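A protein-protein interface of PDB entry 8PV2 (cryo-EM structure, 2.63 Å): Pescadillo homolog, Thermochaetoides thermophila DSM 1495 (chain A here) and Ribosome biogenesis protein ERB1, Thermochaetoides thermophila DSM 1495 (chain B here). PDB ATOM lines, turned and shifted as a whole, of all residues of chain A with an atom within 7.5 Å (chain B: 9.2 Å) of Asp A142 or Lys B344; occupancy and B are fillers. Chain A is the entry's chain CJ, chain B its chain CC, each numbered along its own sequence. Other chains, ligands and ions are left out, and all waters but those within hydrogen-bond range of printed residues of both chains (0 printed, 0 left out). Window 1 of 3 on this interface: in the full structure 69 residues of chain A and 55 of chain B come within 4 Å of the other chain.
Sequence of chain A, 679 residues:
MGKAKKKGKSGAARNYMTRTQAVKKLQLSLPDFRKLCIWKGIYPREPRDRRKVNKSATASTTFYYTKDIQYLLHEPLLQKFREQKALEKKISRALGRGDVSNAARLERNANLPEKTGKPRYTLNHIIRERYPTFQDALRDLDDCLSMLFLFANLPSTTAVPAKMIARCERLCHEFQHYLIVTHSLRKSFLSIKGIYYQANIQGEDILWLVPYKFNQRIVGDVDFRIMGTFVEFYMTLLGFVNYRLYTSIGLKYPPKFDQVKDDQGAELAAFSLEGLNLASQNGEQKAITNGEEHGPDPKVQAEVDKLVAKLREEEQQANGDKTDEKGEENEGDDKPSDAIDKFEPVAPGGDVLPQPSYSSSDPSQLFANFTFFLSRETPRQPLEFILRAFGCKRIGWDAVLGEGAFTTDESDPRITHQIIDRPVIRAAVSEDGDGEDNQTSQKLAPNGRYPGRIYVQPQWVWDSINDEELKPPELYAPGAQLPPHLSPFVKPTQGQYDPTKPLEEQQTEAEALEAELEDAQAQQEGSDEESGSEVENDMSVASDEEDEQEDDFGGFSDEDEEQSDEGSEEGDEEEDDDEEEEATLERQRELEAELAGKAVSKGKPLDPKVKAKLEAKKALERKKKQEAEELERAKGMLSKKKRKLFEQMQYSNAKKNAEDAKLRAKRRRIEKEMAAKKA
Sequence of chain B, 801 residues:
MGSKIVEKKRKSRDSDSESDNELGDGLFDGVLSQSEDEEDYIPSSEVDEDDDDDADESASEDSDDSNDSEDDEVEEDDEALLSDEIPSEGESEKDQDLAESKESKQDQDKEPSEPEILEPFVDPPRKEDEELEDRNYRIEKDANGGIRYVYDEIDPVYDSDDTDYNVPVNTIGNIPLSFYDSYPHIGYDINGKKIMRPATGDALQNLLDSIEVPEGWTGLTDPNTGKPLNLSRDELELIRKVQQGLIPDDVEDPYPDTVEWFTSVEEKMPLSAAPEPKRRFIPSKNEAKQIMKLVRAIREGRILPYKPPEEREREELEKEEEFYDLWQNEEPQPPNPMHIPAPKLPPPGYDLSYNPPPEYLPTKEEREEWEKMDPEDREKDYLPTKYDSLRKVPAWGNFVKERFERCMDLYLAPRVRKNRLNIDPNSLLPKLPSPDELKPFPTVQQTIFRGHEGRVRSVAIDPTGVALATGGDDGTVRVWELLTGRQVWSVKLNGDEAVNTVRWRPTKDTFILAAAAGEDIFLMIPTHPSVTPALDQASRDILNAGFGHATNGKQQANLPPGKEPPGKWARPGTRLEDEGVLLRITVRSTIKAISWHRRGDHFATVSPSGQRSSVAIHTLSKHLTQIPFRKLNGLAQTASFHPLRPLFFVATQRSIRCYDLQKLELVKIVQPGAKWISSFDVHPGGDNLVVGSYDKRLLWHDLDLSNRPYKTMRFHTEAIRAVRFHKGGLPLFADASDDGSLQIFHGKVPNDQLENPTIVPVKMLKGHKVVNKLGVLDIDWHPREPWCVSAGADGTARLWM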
ATOM      1  N   ALA A 137     -23.152  20.025  -9.999  1.00  0.00           N
ATOM      2  CA  ALA A 137     -23.315  18.632  -9.596  1.00  0.00           C
ATOM      3  C   ALA A 137     -23.002  18.443  -8.116  1.00  0.00           C
ATOM      4  O   ALA A 137     -23.706  17.706  -7.417  1.00  0.00           O
ATOM      5  CB  ALA A 137     -22.427  17.730 -10.450  1.00  0.00           C
ATOM      6  N   LEU A 138     -21.955  19.109  -7.623  1.00  0.00           N
ATOM      7  CA  LEU A 138     -21.607  19.018  -6.208  1.00  0.00           C
ATOM      8  C   LEU A 138     -22.633  19.721  -5.328  1.00  0.00           C
ATOM      9  O   LEU A 138     -22.891  19.284  -4.201  1.00  0.00           O
ATOM     10  CB  LEU A 138     -20.214  19.597  -5.963  1.00  0.00           C
ATOM     11  CG  LEU A 138     -19.035  18.856  -6.587  1.00  0.00           C
ATOM     12  CD1 LEU A 138     -17.750  19.630  -6.372  1.00  0.00           C
ATOM     13  CD2 LEU A 138     -18.924  17.458  -6.009  1.00  0.00           C
ATOM     14  N   ARG A 139     -23.205  20.829  -5.812  1.00  0.00           N
ATOM     15  CA  ARG A 139     -24.251  21.509  -5.055  1.00  0.00           C
ATOM     16  C   ARG A 139     -25.477  20.625  -4.895  1.00  0.00           C
ATOM     17  O   ARG A 139     -26.105  20.606  -3.830  1.00  0.00           O
ATOM     18  CB  ARG A 139     -24.642  22.829  -5.722  1.00  0.00           C
ATOM     19  CG  ARG A 139     -23.625  23.942  -5.583  1.00  0.00           C
ATOM     20  CD  ARG A 139     -23.673  24.872  -6.782  1.00  0.00           C
ATOM     21  NE  ARG A 139     -22.517  25.757  -6.835  1.00  0.00           N
ATOM     22  CZ  ARG A 139     -22.290  26.632  -7.804  1.00  0.00           C
ATOM     23  NH1 ARG A 139     -23.126  26.772  -8.819  1.00  0.00           N
ATOM     24  NH2 ARG A 139     -21.197  27.388  -7.753  1.00  0.00           N
ATOM     25  N   ASP A 140     -25.835  19.879  -5.938  1.00  0.00           N
ATOM     26  CA  ASP A 140     -26.969  18.959  -5.831  1.00  0.00           C
ATOM     27  C   ASP A 140     -26.466  17.546  -5.520  1.00  0.00           C
ATOM     28  O   ASP A 140     -26.314  16.692  -6.394  1.00  0.00           O
ATOM     29  CB  ASP A 140     -27.810  18.994  -7.098  1.00  0.00           C
ATOM     30  CG  ASP A 140     -29.128  18.266  -6.936  1.00  0.00           C
ATOM     31  OD1 ASP A 140     -29.576  18.102  -5.781  1.00  0.00           O
ATOM     32  OD2 ASP A 140     -29.721  17.861  -7.955  1.00  0.00           O
ATOM     33  N   LEU A 141     -26.207  17.312  -4.228  1.00  0.00           N
ATOM     34  CA  LEU A 141     -25.826  15.994  -3.733  1.00  0.00           C
ATOM     35  C   LEU A 141     -26.528  15.572  -2.452  1.00  0.00           C
ATOM     36  O   LEU A 141     -26.431  14.397  -2.084  1.00  0.00           O
ATOM     37  CB  LEU A 141     -24.312  15.913  -3.486  1.00  0.00           C
ATOM     38  CG  LEU A 141     -23.334  16.002  -4.654  1.00  0.00           C
ATOM     39  CD1 LEU A 141     -21.911  15.875  -4.149  1.00  0.00           C
ATOM     40  CD2 LEU A 141     -23.630  14.904  -5.655  1.00  0.00           C
ATOM     41  N   ASP A 142     -27.211  16.488  -1.761  1.00  0.00           N
ATOM     42  CA  ASP A 142     -27.790  16.181  -0.454  1.00  0.00           C
ATOM     43  C   ASP A 142     -28.878  15.119  -0.566  1.00  0.00           C
ATOM     44  O   ASP A 142     -28.860  14.101   0.140  1.00  0.00           O
ATOM     45  CB  ASP A 142     -28.357  17.458   0.167  1.00  0.00           C
ATOM     46  CG  ASP A 142     -27.279  18.442   0.559  1.00  0.00           C
ATOM     47  OD1 ASP A 142     -26.159  17.999   0.877  1.00  0.00           O
ATOM     48  OD2 ASP A 142     -27.553  19.661   0.552  1.00  0.00           O
ATOM     49  N   ASP A 143     -29.830  15.350  -1.474  1.00  0.00           N
ATOM     50  CA  ASP A 143     -30.913  14.399  -1.697  1.00  0.00           C
ATOM     51  C   ASP A 143     -30.383  13.089  -2.261  1.00  0.00           C
ATOM     52  O   ASP A 143     -30.894  12.015  -1.929  1.00  0.00           O
ATOM     53  CB  ASP A 143     -31.947  15.006  -2.642  1.00  0.00           C
ATOM     54  CG  ASP A 143     -32.669  16.183  -2.028  1.00  0.00           C
ATOM     55  OD1 ASP A 143     -32.826  16.209  -0.790  1.00  0.00           O
ATOM     56  OD2 ASP A 143     -33.075  17.090  -2.784  1.00  0.00           O
ATOM     57  N   CYS A 144     -29.352  13.167  -3.109  1.00  0.00           N
ATOM     58  CA  CYS A 144     -28.723  11.970  -3.658  1.00  0.00           C
ATOM     59  C   CYS A 144     -28.163  11.078  -2.560  1.00  0.00           C
ATOM     60  O   CYS A 144     -28.460   9.875  -2.508  1.00  0.00           O
ATOM     61  CB  CYS A 144     -27.609  12.376  -4.622  1.00  0.00           C
ATOM     62  SG  CYS A 144     -26.658  11.006  -5.299  1.00  0.00           S
ATOM     63  N   LEU A 145     -27.363  11.658  -1.664  1.00  0.00           N
ATOM     64  CA  LEU A 145     -26.731  10.869  -0.618  1.00  0.00           C
ATOM     65  C   LEU A 145     -27.756  10.350   0.381  1.00  0.00           C
ATOM     66  O   LEU A 145     -27.670   9.195   0.814  1.00  0.00           O
ATOM     67  CB  LEU A 145     -25.643  11.690   0.066  1.00  0.00           C
ATOM     68  CG  LEU A 145     -24.523  12.029  -0.920  1.00  0.00           C
ATOM     69  CD1 LEU A 145     -23.646  13.168  -0.421  1.00  0.00           C
ATOM     70  CD2 LEU A 145     -23.697  10.794  -1.240  1.00  0.00           C
ATOM     71  N   SER A 146     -28.757  11.170   0.731  1.00  0.00           N
ATOM     72  CA  SER A 146     -29.804  10.693   1.634  1.00  0.00           C
ATOM     73  C   SER A 146     -30.590   9.539   1.020  1.00  0.00           C
ATOM     74  O   SER A 146     -30.845   8.528   1.691  1.00  0.00           O
ATOM     75  CB  SER A 146     -30.739  11.840   2.014  1.00  0.00           C
ATOM     76  OG  SER A 146     -30.008  12.988   2.403  1.00  0.00           O
ATOM     77  N   MET A 147     -30.930   9.651  -0.270  1.00  0.00           N
ATOM     78  CA  MET A 147     -31.643   8.590  -0.972  1.00  0.00           C
ATOM     79  C   MET A 147     -30.849   7.295  -0.992  1.00  0.00           C
ATOM     80  O   MET A 147     -31.379   6.222  -0.671  1.00  0.00           O
ATOM     81  CB  MET A 147     -31.923   9.028  -2.407  1.00  0.00           C
ATOM     82  CG  MET A 147     -32.762   8.054  -3.193  1.00  0.00           C
ATOM     83  SD  MET A 147     -34.383   7.930  -2.455  1.00  0.00           S
ATOM     84  CE  MET A 147     -34.991   9.515  -2.959  1.00  0.00           C
ATOM     85  N   LEU A 148     -29.570   7.375  -1.357  1.00  0.00           N
ATOM     86  CA  LEU A 148     -28.811   6.152  -1.577  1.00  0.00           C
ATOM     87  C   LEU A 148     -28.412   5.500  -0.262  1.00  0.00           C
ATOM     88  O   LEU A 148     -28.339   4.271  -0.173  1.00  0.00           O
ATOM     89  CB  LEU A 148     -27.601   6.436  -2.463  1.00  0.00           C
ATOM     90  CG  LEU A 148     -28.017   6.731  -3.908  1.00  0.00           C
ATOM     91  CD1 LEU A 148     -26.833   6.666  -4.833  1.00  0.00           C
ATOM     92  CD2 LEU A 148     -29.102   5.770  -4.398  1.00  0.00           C
ATOM     93  N   TYR A 197     -24.115  14.433   8.299  1.00  0.00           N
ATOM     94  CA  TYR A 197     -22.723  14.642   7.922  1.00  0.00           C
ATOM     95  C   TYR A 197     -22.647  15.803   6.947  1.00  0.00           C
ATOM     96  O   TYR A 197     -23.388  15.831   5.958  1.00  0.00           O
ATOM     97  CB  TYR A 197     -22.113  13.388   7.286  1.00  0.00           C
ATOM     98  CG  TYR A 197     -21.917  12.204   8.213  1.00  0.00           C
ATOM     99  CD1 TYR A 197     -21.981  12.349   9.592  1.00  0.00           C
ATOM    100  CD2 TYR A 197     -21.667  10.938   7.700  1.00  0.00           C
ATOM    101  CE1 TYR A 197     -21.802  11.267  10.433  1.00  0.00           C
ATOM    102  CE2 TYR A 197     -21.488   9.851   8.533  1.00  0.00           C
ATOM    103  CZ  TYR A 197     -21.556  10.020   9.897  1.00  0.00           C
ATOM    104  OH  TYR A 197     -21.376   8.940  10.730  1.00  0.00           O
ATOM    105  N   GLN A 198     -21.765  16.758   7.229  1.00  0.00           N
ATOM    106  CA  GLN A 198     -21.497  17.875   6.338  1.00  0.00           C
ATOM    107  C   GLN A 198     -20.041  17.828   5.905  1.00  0.00           C
ATOM    108  O   GLN A 198     -19.132  17.911   6.742  1.00  0.00           O
ATOM    109  CB  GLN A 198     -21.796  19.220   7.003  1.00  0.00           C
ATOM    110  CG  GLN A 198     -21.467  20.410   6.114  1.00  0.00           C
ATOM    111  CD  GLN A 198     -21.683  21.736   6.807  1.00  0.00           C
ATOM    112  OE1 GLN A 198     -22.096  21.784   7.961  1.00  0.00           O
ATOM    113  NE2 GLN A 198     -21.401  22.825   6.102  1.00  0.00           N
ATOM    114  N   ALA A 199     -19.833  17.717   4.597  1.00  0.00           N
ATOM    115  CA  ALA A 199     -18.513  17.701   3.994  1.00  0.00           C
ATOM    116  C   ALA A 199     -18.393  18.852   3.009  1.00  0.00           C
ATOM    117  O   ALA A 199     -19.349  19.194   2.310  1.00  0.00           O
ATOM    118  CB  ALA A 199     -18.237  16.378   3.275  1.00  0.00           C
ATOM    119  N   ASP A 205     -20.625  22.907   0.422  1.00  0.00           N
ATOM    120  CA  ASP A 205     -21.049  22.192   1.616  1.00  0.00           C
ATOM    121  C   ASP A 205     -22.208  21.260   1.295  1.00  0.00           C
ATOM    122  O   ASP A 205     -23.226  21.676   0.737  1.00  0.00           O
ATOM    123  CB  ASP A 205     -21.456  23.179   2.708  1.00  0.00           C
ATOM    124  N   ILE A 206     -22.051  19.989   1.653  1.00  0.00           N
ATOM    125  CA  ILE A 206     -23.071  18.975   1.428  1.00  0.00           C
ATOM    126  C   ILE A 206     -23.390  18.320   2.761  1.00  0.00           C
ATOM    127  O   ILE A 206     -22.492  17.791   3.424  1.00  0.00           O
ATOM    128  CB  ILE A 206     -22.615  17.919   0.404  1.00  0.00           C
ATOM    129  N   LEU A 207     -24.661  18.355   3.151  1.00  0.00           N
ATOM    130  CA  LEU A 207     -25.118  17.764   4.400  1.00  0.00           C
ATOM    131  C   LEU A 207     -26.178  16.716   4.099  1.00  0.00           C
ATOM    132  O   LEU A 207     -27.162  17.002   3.412  1.00  0.00           O
ATOM    133  CB  LEU A 207     -25.680  18.830   5.344  1.00  0.00           C
ATOM    134  N   TRP A 208     -25.979  15.511   4.623  1.00  0.00           N
ATOM    135  CA  TRP A 208     -26.916  14.420   4.391  1.00  0.00           C
ATOM    136  C   TRP A 208     -27.195  13.679   5.687  1.00  0.00           C
ATOM    137  O   TRP A 208     -26.432  13.769   6.651  1.00  0.00           O
ATOM    138  CB  TRP A 208     -26.402  13.429   3.343  1.00  0.00           C
ATOM    139  CG  TRP A 208     -25.115  12.762   3.702  1.00  0.00           C
ATOM    140  CD1 TRP A 208     -24.959  11.533   4.272  1.00  0.00           C
ATOM    141  CD2 TRP A 208     -23.798  13.274   3.487  1.00  0.00           C
ATOM    142  NE1 TRP A 208     -23.626  11.255   4.437  1.00  0.00           N
ATOM    143  CE2 TRP A 208     -22.892  12.309   3.961  1.00  0.00           C
ATOM    144  CE3 TRP A 208     -23.298  14.461   2.945  1.00  0.00           C
ATOM    145  CZ2 TRP A 208     -21.514  12.492   3.906  1.00  0.00           C
ATOM    146  CZ3 TRP A 208     -21.931  14.641   2.893  1.00  0.00           C
ATOM    147  CH2 TRP A 208     -21.056  13.665   3.373  1.00  0.00           C
ATOM    148  N   LEU A 209     -28.295  12.931   5.691  1.00  0.00           N
ATOM    149  CA  LEU A 209     -28.737  12.185   6.858  1.00  0.00           C
ATOM    150  C   LEU A 209     -28.480  10.706   6.603  1.00  0.00           C
ATOM    151  O   LEU A 209     -28.659  10.226   5.479  1.00  0.00           O
ATOM    152  CB  LEU A 209     -30.225  12.418   7.135  1.00  0.00           C
ATOM    153  CG  LEU A 209     -30.863  11.964   8.458  1.00  0.00           C
ATOM    154  CD1 LEU A 209     -32.089  12.812   8.697  1.00  0.00           C
ATOM    155  CD2 LEU A 209     -31.214  10.496   8.585  1.00  0.00           C
ATOM    156  N   TYR A 234     -30.084   8.920  -9.061  1.00  0.00           N
ATOM    157  CA  TYR A 234     -29.052   9.288  -8.098  1.00  0.00           C
ATOM    158  C   TYR A 234     -27.881   8.317  -8.134  1.00  0.00           C
ATOM    159  O   TYR A 234     -26.744   8.710  -7.867  1.00  0.00           O
ATOM    160  CB  TYR A 234     -29.631   9.389  -6.688  1.00  0.00           C
ATOM    161  CG  TYR A 234     -30.543  10.578  -6.489  1.00  0.00           C
ATOM    162  CD1 TYR A 234     -30.192  11.828  -6.975  1.00  0.00           C
ATOM    163  CD2 TYR A 234     -31.717  10.468  -5.754  1.00  0.00           C
ATOM    164  CE1 TYR A 234     -31.005  12.920  -6.788  1.00  0.00           C
ATOM    165  CE2 TYR A 234     -32.539  11.556  -5.559  1.00  0.00           C
ATOM    166  CZ  TYR A 234     -32.175  12.780  -6.077  1.00  0.00           C
ATOM    167  OH  TYR A 234     -32.984  13.874  -5.885  1.00  0.00           O
ATOM    168  N   PRO B 341     -34.802  26.878  -8.561  1.00  0.00           N
ATOM    169  CA  PRO B 341     -34.260  25.777  -7.760  1.00  0.00           C
ATOM    170  C   PRO B 341     -35.248  25.311  -6.703  1.00  0.00           C
ATOM    171  O   PRO B 341     -36.097  26.066  -6.226  1.00  0.00           O
ATOM    172  CB  PRO B 341     -33.010  26.390  -7.123  1.00  0.00           C
ATOM    173  CG  PRO B 341     -33.294  27.849  -7.099  1.00  0.00           C
ATOM    174  CD  PRO B 341     -34.037  28.118  -8.369  1.00  0.00           C
ATOM    175  N   ALA B 342     -35.130  24.033  -6.357  1.00  0.00           N
ATOM    176  CA  ALA B 342     -36.020  23.429  -5.381  1.00  0.00           C
ATOM    177  C   ALA B 342     -35.781  24.031  -3.999  1.00  0.00           C
ATOM    178  O   ALA B 342     -34.668  24.460  -3.686  1.00  0.00           O
ATOM    179  CB  ALA B 342     -35.810  21.918  -5.333  1.00  0.00           C
ATOM    180  N   PRO B 343     -36.819  24.105  -3.164  1.00  0.00           N
ATOM    181  CA  PRO B 343     -36.617  24.579  -1.791  1.00  0.00           C
ATOM    182  C   PRO B 343     -35.761  23.607  -0.995  1.00  0.00           C
ATOM    183  O   PRO B 343     -36.095  22.430  -0.844  1.00  0.00           O
ATOM    184  CB  PRO B 343     -38.042  24.665  -1.233  1.00  0.00           C
ATOM    185  CG  PRO B 343     -38.845  23.754  -2.094  1.00  0.00           C
ATOM    186  CD  PRO B 343     -38.242  23.866  -3.457  1.00  0.00           C
ATOM    187  N   LYS B 344     -34.646  24.116  -0.487  1.00  0.00           N
ATOM    188  CA  LYS B 344     -33.686  23.325   0.266  1.00  0.00           C
ATOM    189  C   LYS B 344     -34.240  23.081   1.661  1.00  0.00           C
ATOM    190  O   LYS B 344     -34.890  23.962   2.234  1.00  0.00           O
ATOM    191  CB  LYS B 344     -32.336  24.042   0.337  1.00  0.00           C
ATOM    192  CG  LYS B 344     -31.213  23.219   0.936  1.00  0.00           C
ATOM    193  CD  LYS B 344     -29.865  23.863   0.661  1.00  0.00           C
ATOM    194  CE  LYS B 344     -28.722  22.935   1.033  1.00  0.00           C
ATOM    195  NZ  LYS B 344     -27.402  23.497   0.637  1.00  0.00           N
ATOM    196  N   LEU B 345     -34.011  21.882   2.186  1.00  0.00           N
ATOM    197  CA  LEU B 345     -34.451  21.568   3.535  1.00  0.00           C
ATOM    198  C   LEU B 345     -33.687  22.424   4.543  1.00  0.00           C
ATOM    199  O   LEU B 345     -32.506  22.726   4.331  1.00  0.00           O
ATOM    200  CB  LEU B 345     -34.245  20.085   3.839  1.00  0.00           C
ATOM    201  CG  LEU B 345     -35.140  19.109   3.077  1.00  0.00           C
ATOM    202  CD1 LEU B 345     -34.748  17.672   3.377  1.00  0.00           C
ATOM    203  CD2 LEU B 345     -36.598  19.352   3.429  1.00  0.00           C
ATOM    204  N   PRO B 346     -34.334  22.858   5.629  1.00  0.00           N
ATOM    205  CA  PRO B 346     -33.635  23.683   6.612  1.00  0.00           C
ATOM    206  C   PRO B 346     -32.569  22.883   7.329  1.00  0.00           C
ATOM    207  O   PRO B 346     -32.682  21.652   7.472  1.00  0.00           O
ATOM    208  CB  PRO B 346     -34.757  24.113   7.575  1.00  0.00           C
ATOM    209  CG  PRO B 346     -36.028  23.878   6.824  1.00  0.00           C
ATOM    210  CD  PRO B 346     -35.757  22.693   5.960  1.00  0.00           C
ATOM    211  N   PRO B 347     -31.493  23.529   7.779  1.00  0.00           N
ATOM    212  CA  PRO B 347     -30.481  22.816   8.549  1.00  0.00           C
ATOM    213  C   PRO B 347     -31.036  22.385   9.889  1.00  0.00           C
ATOM    214  O   PRO B 347     -31.968  23.013  10.428  1.00  0.00           O
ATOM    215  CB  PRO B 347     -29.361  23.853   8.705  1.00  0.00           C
ATOM    216  CG  PRO B 347     -30.034  25.167   8.535  1.00  0.00           C
ATOM    217  CD  PRO B 347     -31.120  24.933   7.536  1.00  0.00           C
ATOM    218  N   ARG B 403     -38.908  11.032   3.445  1.00  0.00           N
ATOM    219  CA  ARG B 403     -38.160  11.047   2.192  1.00  0.00           C
ATOM    220  C   ARG B 403     -39.092  10.841   1.004  1.00  0.00           C
ATOM    221  O   ARG B 403     -38.867  11.400  -0.073  1.00  0.00           O
ATOM    222  CB  ARG B 403     -37.057   9.990   2.221  1.00  0.00           C
ATOM    223  CG  ARG B 403     -36.082  10.071   1.060  1.00  0.00           C
ATOM    224  CD  ARG B 403     -35.387  11.422   1.032  1.00  0.00           C
ATOM    225  NE  ARG B 403     -34.661  11.696   2.265  1.00  0.00           N
ATOM    226  CZ  ARG B 403     -34.214  12.894   2.616  1.00  0.00           C
ATOM    227  NH1 ARG B 403     -34.413  13.956   1.854  1.00  0.00           N
ATOM    228  NH2 ARG B 403     -33.556  13.032   3.764  1.00  0.00           N
ATOM    229  N   ARG B 406     -40.502  14.132   0.395  1.00  0.00           N
ATOM    230  CA  ARG B 406     -39.509  14.951  -0.294  1.00  0.00           C
ATOM    231  C   ARG B 406     -39.459  14.612  -1.781  1.00  0.00           C
ATOM    232  O   ARG B 406     -39.331  15.506  -2.630  1.00  0.00           O
ATOM    233  CB  ARG B 406     -38.135  14.761   0.346  1.00  0.00           C
ATOM    234  CG  ARG B 406     -36.985  15.490  -0.336  1.00  0.00           C
ATOM    235  CD  ARG B 406     -37.160  16.989  -0.240  1.00  0.00           C
ATOM    236  NE  ARG B 406     -36.049  17.721  -0.833  1.00  0.00           N
ATOM    237  CZ  ARG B 406     -36.039  19.034  -1.002  1.00  0.00           C
ATOM    238  NH1 ARG B 406     -37.071  19.781  -0.649  1.00  0.00           N
ATOM    239  NH2 ARG B 406     -34.966  19.613  -1.530  1.00  0.00           N
ATOM    240  N   LEU B 410     -40.350  17.206  -4.842  1.00  0.00           N
ATOM    241  CA  LEU B 410     -39.393  17.557  -5.890  1.00  0.00           C
ATOM    242  C   LEU B 410     -40.017  17.693  -7.278  1.00  0.00           C
ATOM    243  O   LEU B 410     -39.631  18.588  -8.036  1.00  0.00           O
ATOM    244  CB  LEU B 410     -38.249  16.544  -5.936  1.00  0.00           C
ATOM    245  CG  LEU B 410     -37.193  16.704  -4.838  1.00  0.00           C
ATOM    246  CD1 LEU B 410     -36.026  15.759  -5.059  1.00  0.00           C
ATOM    247  CD2 LEU B 410     -36.707  18.141  -4.760  1.00  0.00           C
ATOM    248  N   ARG B 415     -43.258  25.225  -8.110  1.00  0.00           N
ATOM    249  CA  ARG B 415     -42.159  26.076  -7.680  1.00  0.00           C
ATOM    250  C   ARG B 415     -42.455  27.515  -8.073  1.00  0.00           C
ATOM    251  O   ARG B 415     -42.685  27.808  -9.250  1.00  0.00           O
ATOM    252  CB  ARG B 415     -40.836  25.612  -8.287  1.00  0.00           C
ATOM    253  CG  ARG B 415     -40.381  24.267  -7.764  1.00  0.00           C
ATOM    254  CD  ARG B 415     -38.955  23.964  -8.156  1.00  0.00           C
ATOM    255  NE  ARG B 415     -38.695  22.531  -8.153  1.00  0.00           N
ATOM    256  CZ  ARG B 415     -37.586  21.975  -8.618  1.00  0.00           C
ATOM    257  NH1 ARG B 415     -36.608  22.706  -9.124  1.00  0.00           N
ATOM    258  NH2 ARG B 415     -37.457  20.654  -8.576  1.00  0.00           N
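Among the printed residues, merely in contact across the chains: Ser A146 with Arg B403 (3.5 Å), Tyr A234 with Leu B410 (3.7 Å) and Asp A143 with Leu B410 (3.96 Å).
Asp A142 touches one residue of chain B.
Of chain B, only Arg B403, Arg B406 and Leu B410 come within 4 Å of Asp A143.
Of the printed residues of chain B, Ser A146 touches Arg B403.
Ala A199 touches none of the printed residues of chain B.
No residue of chain B comes within 4 Å of Ile A206.
Leu A207 touches none of the printed residues of chain B.
Printed residues of chain B within 4 Å of Tyr A234: Leu B410.
Of the printed residues of chain A, Arg B403 touches Asp A143 and Ser A146.
Of the printed residues of chain A, Arg B406 touches Asp A143 (3.4 Å).
Of the printed residues of chain A, Leu B410 touches Asp A143 (3.96 Å) and Tyr A234 (3.7 Å).
The nearest residue of chain B that does not touch Asp A142 is Arg B403 (5.8 Å).
The nearest residue of chain A that does not touch Lys B344 is Asp A205 (4.6 Å).
The nearest printed residue of chain B that does not touch Ser A146 is Leu B345 (6.7 Å).
The guanidinium group (NH1) of Arg B403 is in salt-bridge range of the side-chain carboxylate (OD1) of Asp A143 (3.8 Å).
The guanidinium group of Arg B406 lies within salt-bridge range of the side-chain carboxylate of Asp A143 (3.4 Å).
The side-chain carboxylate (OD2) of Asp A142 lies within salt-bridge range of the side-chain amino group (NZ) of Lys B344 (3.8 Å).
Of the 11 printed residues of chain B, 4 touch a printed residue of chain A.
Printed residues of chain B that touch a printed residue of chain A: Lys B344, Arg B403, Arg B406 and Leu B410.
Among the printed residues, 6 pairs touch across the chains.
The backbone carbonyl oxygen of Tyr A234 lies within hydrogen-bond range of the side-chain sulfur of Cys A144 (3.4 Å).
O of Pro B343 sits at hydrogen-bond distance from NH1 of Arg B406, at 2.8 Å.
O of Asp A142 sits at hydrogen-bond distance from OG of Ser A146.
The side-chain carboxylate (OD1) of Asp A142 lies within hydrogen-bond range of the backbone NH (N) of Leu A207 (2.7 Å).
The backbone carbonyl oxygen (O) of Leu B410 lies within hydrogen-bond range of the guanidinium group (NH2) of Arg B415 (3.0 Å).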
